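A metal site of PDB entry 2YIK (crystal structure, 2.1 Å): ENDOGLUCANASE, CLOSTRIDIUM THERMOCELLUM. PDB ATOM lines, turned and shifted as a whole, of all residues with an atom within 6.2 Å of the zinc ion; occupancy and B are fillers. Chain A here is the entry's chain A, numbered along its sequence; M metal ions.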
ATOM      1  N   ASN A  54      30.872 -29.945 -23.541  1.00  0.00           N
ATOM      2  CA  ASN A  54      29.476 -29.563 -23.769  1.00  0.00           C
ATOM      3  C   ASN A  54      28.788 -28.861 -22.603  1.00  0.00           C
ATOM      4  O   ASN A  54      27.588 -28.596 -22.676  1.00  0.00           O
ATOM      5  CB  ASN A  54      28.626 -30.780 -24.183  1.00  0.00           C
ATOM      6  CG  ASN A  54      28.763 -31.137 -25.657  1.00  0.00           C
ATOM      7  OD1 ASN A  54      27.833 -31.658 -26.274  1.00  0.00           O
ATOM      8  ND2 ASN A  54      29.937 -30.877 -26.213  1.00  0.00           N
ATOM      9  N   MET A  55      29.519 -28.573 -21.533  1.00  0.00           N
ATOM     10  CA  MET A  55      28.915 -27.879 -20.398  1.00  0.00           C
ATOM     11  C   MET A  55      28.358 -26.528 -20.869  1.00  0.00           C
ATOM     12  O   MET A  55      28.965 -25.822 -21.661  1.00  0.00           O
ATOM     13  CB  MET A  55      29.933 -27.693 -19.279  1.00  0.00           C
ATOM     14  CG  MET A  55      30.247 -29.006 -18.582  1.00  0.00           C
ATOM     15  SD  MET A  55      31.407 -28.843 -17.216  1.00  0.00           S
ATOM     16  CE  MET A  55      31.158 -30.423 -16.403  1.00  0.00           C
ATOM     17  N   CYS A  56      27.200 -26.166 -20.330  1.00  0.00           N
ATOM     18  CA  CYS A  56      26.502 -24.952 -20.719  1.00  0.00           C
ATOM     19  C   CYS A  56      26.137 -24.086 -19.515  1.00  0.00           C
ATOM     20  O   CYS A  56      26.030 -24.585 -18.389  1.00  0.00           O
ATOM     21  CB  CYS A  56      25.245 -25.373 -21.494  1.00  0.00           C
ATOM     22  SG  CYS A  56      24.167 -24.093 -22.134  1.00  0.00           S
ATOM     23  N   GLY A  57      25.955 -22.785 -19.754  1.00  0.00           N
ATOM     24  CA  GLY A  57      25.552 -21.899 -18.668  1.00  0.00           C
ATOM     25  C   GLY A  57      26.604 -21.055 -17.964  1.00  0.00           C
ATOM     26  O   GLY A  57      27.703 -20.834 -18.470  1.00  0.00           O
ATOM     27  N   ARG A  69      36.825 -23.767 -22.984  1.00  0.00           N
ATOM     28  CA  ARG A  69      35.376 -23.653 -22.760  1.00  0.00           C
ATOM     29  C   ARG A  69      35.115 -22.656 -21.632  1.00  0.00           C
ATOM     30  O   ARG A  69      35.721 -22.740 -20.557  1.00  0.00           O
ATOM     31  CB  ARG A  69      34.746 -24.998 -22.372  1.00  0.00           C
ATOM     32  CG  ARG A  69      34.484 -25.984 -23.516  1.00  0.00           C
ATOM     33  CD  ARG A  69      33.701 -25.358 -24.659  1.00  0.00           C
ATOM     34  NE  ARG A  69      32.739 -24.351 -24.201  1.00  0.00           N
ATOM     35  CZ  ARG A  69      31.589 -24.605 -23.593  1.00  0.00           C
ATOM     36  NH1 ARG A  69      31.226 -25.864 -23.348  1.00  0.00           N
ATOM     37  NH2 ARG A  69      30.810 -23.605 -23.210  1.00  0.00           N
ATOM     38  N   ASP A  71      31.855 -19.799 -19.846  1.00  0.00           N
ATOM     39  CA  ASP A  71      30.415 -19.654 -19.682  1.00  0.00           C
ATOM     40  C   ASP A  71      29.751 -19.342 -21.012  1.00  0.00           C
ATOM     41  O   ASP A  71      30.281 -18.580 -21.807  1.00  0.00           O
ATOM     42  CB  ASP A  71      30.090 -18.537 -18.679  1.00  0.00           C
ATOM     43  CG  ASP A  71      30.539 -18.867 -17.278  1.00  0.00           C
ATOM     44  OD1 ASP A  71      30.903 -20.027 -17.027  1.00  0.00           O
ATOM     45  OD2 ASP A  71      30.518 -17.963 -16.408  1.00  0.00           O
ATOM     46  N   CYS A  72      28.577 -19.919 -21.242  1.00  0.00           N
ATOM     47  CA  CYS A  72      27.852 -19.684 -22.495  1.00  0.00           C
ATOM     48  C   CYS A  72      26.351 -19.621 -22.281  1.00  0.00           C
ATOM     49  O   CYS A  72      25.834 -20.136 -21.285  1.00  0.00           O
ATOM     50  CB  CYS A  72      28.170 -20.801 -23.490  1.00  0.00           C
ATOM     51  SG  CYS A  72      27.839 -22.451 -22.827  1.00  0.00           S
ATOM     52  N   HIS A  73      25.657 -19.016 -23.242  1.00  0.00           N
ATOM     53  CA  HIS A  73      24.208 -18.856 -23.197  1.00  0.00           C
ATOM     54  C   HIS A  73      23.787 -18.467 -21.787  1.00  0.00           C
ATOM     55  O   HIS A  73      22.792 -18.979 -21.262  1.00  0.00           O
ATOM     56  CB  HIS A  73      23.522 -20.161 -23.623  1.00  0.00           C
ATOM     57  CG  HIS A  73      24.057 -20.720 -24.903  1.00  0.00           C
ATOM     58  ND1 HIS A  73      24.940 -21.785 -24.954  1.00  0.00           N
ATOM     59  CD2 HIS A  73      23.900 -20.299 -26.187  1.00  0.00           C
ATOM     60  CE1 HIS A  73      25.303 -21.999 -26.206  1.00  0.00           C
ATOM     61  NE2 HIS A  73      24.686 -21.115 -26.973  1.00  0.00           N
ATOM     62  N   ASP A  76      20.294 -17.701 -20.518  1.00  0.00           N
ATOM     63  CA  ASP A  76      19.382 -18.792 -20.170  1.00  0.00           C
ATOM     64  C   ASP A  76      19.001 -18.609 -18.701  1.00  0.00           C
ATOM     65  O   ASP A  76      17.914 -19.003 -18.273  1.00  0.00           O
ATOM     66  CB  ASP A  76      20.067 -20.175 -20.270  1.00  0.00           C
ATOM     67  CG  ASP A  76      20.271 -20.657 -21.697  1.00  0.00           C
ATOM     68  OD1 ASP A  76      19.755 -20.025 -22.639  1.00  0.00           O
ATOM     69  OD2 ASP A  76      20.953 -21.696 -21.857  1.00  0.00           O
ATOM     70  N   HIS A 115      25.120 -29.118 -23.699  1.00  0.00           N
ATOM     71  CA  HIS A 115      24.653 -28.946 -25.067  1.00  0.00           C
ATOM     72  C   HIS A 115      24.411 -30.379 -25.501  1.00  0.00           C
ATOM     73  O   HIS A 115      25.053 -31.303 -25.017  1.00  0.00           O
ATOM     74  CB  HIS A 115      25.739 -28.352 -25.973  1.00  0.00           C
ATOM     75  CG  HIS A 115      26.188 -27.005 -25.551  1.00  0.00           C
ATOM     76  ND1 HIS A 115      27.526 -26.641 -25.532  1.00  0.00           N
ATOM     77  CD2 HIS A 115      25.510 -25.909 -25.164  1.00  0.00           C
ATOM     78  CE1 HIS A 115      27.634 -25.392 -25.149  1.00  0.00           C
ATOM     79  NE2 HIS A 115      26.424 -24.917 -24.919  1.00  0.00           N
ATOM     80  N   HIS A 120      24.066 -26.635 -29.853  1.00  0.00           N
ATOM     81  CA  HIS A 120      24.012 -26.051 -28.499  1.00  0.00           C
ATOM     82  C   HIS A 120      22.640 -26.145 -27.821  1.00  0.00           C
ATOM     83  O   HIS A 120      22.442 -25.633 -26.705  1.00  0.00           O
ATOM     84  CB  HIS A 120      24.491 -24.573 -28.542  1.00  0.00           C
ATOM     85  CG  HIS A 120      25.862 -24.393 -29.079  1.00  0.00           C
ATOM     86  ND1 HIS A 120      26.930 -25.244 -28.807  1.00  0.00           N
ATOM     87  CD2 HIS A 120      26.418 -23.424 -29.897  1.00  0.00           C
ATOM     88  CE1 HIS A 120      28.021 -24.829 -29.396  1.00  0.00           C
ATOM     89  NE2 HIS A 120      27.725 -23.720 -30.070  1.00  0.00           N
ATOM     90  N   LYS A 122      19.588 -27.859 -25.777  1.00  0.00           N
ATOM     91  CA  LYS A 122      19.543 -28.801 -24.662  1.00  0.00           C
ATOM     92  C   LYS A 122      18.195 -29.503 -24.787  1.00  0.00           C
ATOM     93  O   LYS A 122      17.157 -28.920 -24.471  1.00  0.00           O
ATOM     94  CB  LYS A 122      19.664 -28.069 -23.316  1.00  0.00           C
ATOM     95  CG  LYS A 122      21.000 -27.322 -23.147  1.00  0.00           C
ATOM     96  CD  LYS A 122      21.213 -26.741 -21.746  1.00  0.00           C
ATOM     97  CE  LYS A 122      20.230 -25.616 -21.400  1.00  0.00           C
ATOM     98  NZ  LYS A 122      20.649 -24.871 -20.170  1.00  0.00           N
ATOM     99  N   PRO A 197      30.130 -21.503 -28.520  1.00  0.00           N
ATOM    100  CA  PRO A 197      28.943 -21.256 -27.695  1.00  0.00           C
ATOM    101  C   PRO A 197      29.025 -19.984 -26.838  1.00  0.00           C
ATOM    102  O   PRO A 197      27.998 -19.384 -26.512  1.00  0.00           O
ATOM    103  CB  PRO A 197      28.830 -22.542 -26.866  1.00  0.00           C
ATOM    104  CG  PRO A 197      30.251 -23.001 -26.741  1.00  0.00           C
ATOM    105  CD  PRO A 197      30.798 -22.763 -28.133  1.00  0.00           C
ATOM    106  N   ARG A 204      16.733 -18.523 -27.569  1.00  0.00           N
ATOM    107  CA  ARG A 204      16.712 -19.846 -26.943  1.00  0.00           C
ATOM    108  C   ARG A 204      15.480 -19.978 -26.050  1.00  0.00           C
ATOM    109  O   ARG A 204      15.529 -19.679 -24.857  1.00  0.00           O
ATOM    110  CB  ARG A 204      17.985 -20.076 -26.135  1.00  0.00           C
ATOM    111  CG  ARG A 204      19.212 -20.375 -26.993  1.00  0.00           C
ATOM    112  CD  ARG A 204      20.503 -20.186 -26.222  1.00  0.00           C
ATOM    113  NE  ARG A 204      20.698 -21.178 -25.170  1.00  0.00           N
ATOM    114  CZ  ARG A 204      21.107 -22.429 -25.377  1.00  0.00           C
ATOM    115  NH1 ARG A 204      21.357 -22.855 -26.607  1.00  0.00           N
ATOM    116  NH2 ARG A 204      21.264 -23.255 -24.342  1.00  0.00           N
HETATM  117 ZN    ZN M   1      25.786 -23.155 -23.667  1.00  0.00          ZN
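Merely in contact with the zinc ion: Gly 57 (3.9 Å). Of the 14 residues printed, 5 come within 4 Å of the zinc ion.
O of Asn 54 is in hydrogen-bond range of N of His 115, 2.7 Å away. The backbone carbonyl oxygen (O) of Gly 57 is in hydrogen-bond range of the backbone NH (N) of Cys 72. SG of Cys 72 lies close to O of Met 55 (3.7 Å). The side-chain sulfur (SG) of Cys 72 sits close to the guanidinium group (NH2) of Arg 69 (3.2 Å). The guanidinium group (NH2) of Arg 204 lies close to the side-chain sulfur (SG) of Cys 56.
A ring nitrogen (ND1) of His 73 is bound to the zinc ion (2.1 Å). NE2 of His 115 binds the zinc ion (2.3 Å). SG of Cys 72 binds the zinc ion (2.3 Å). The zinc ion is bound by SG of Cys 56, at 2.4 Å.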
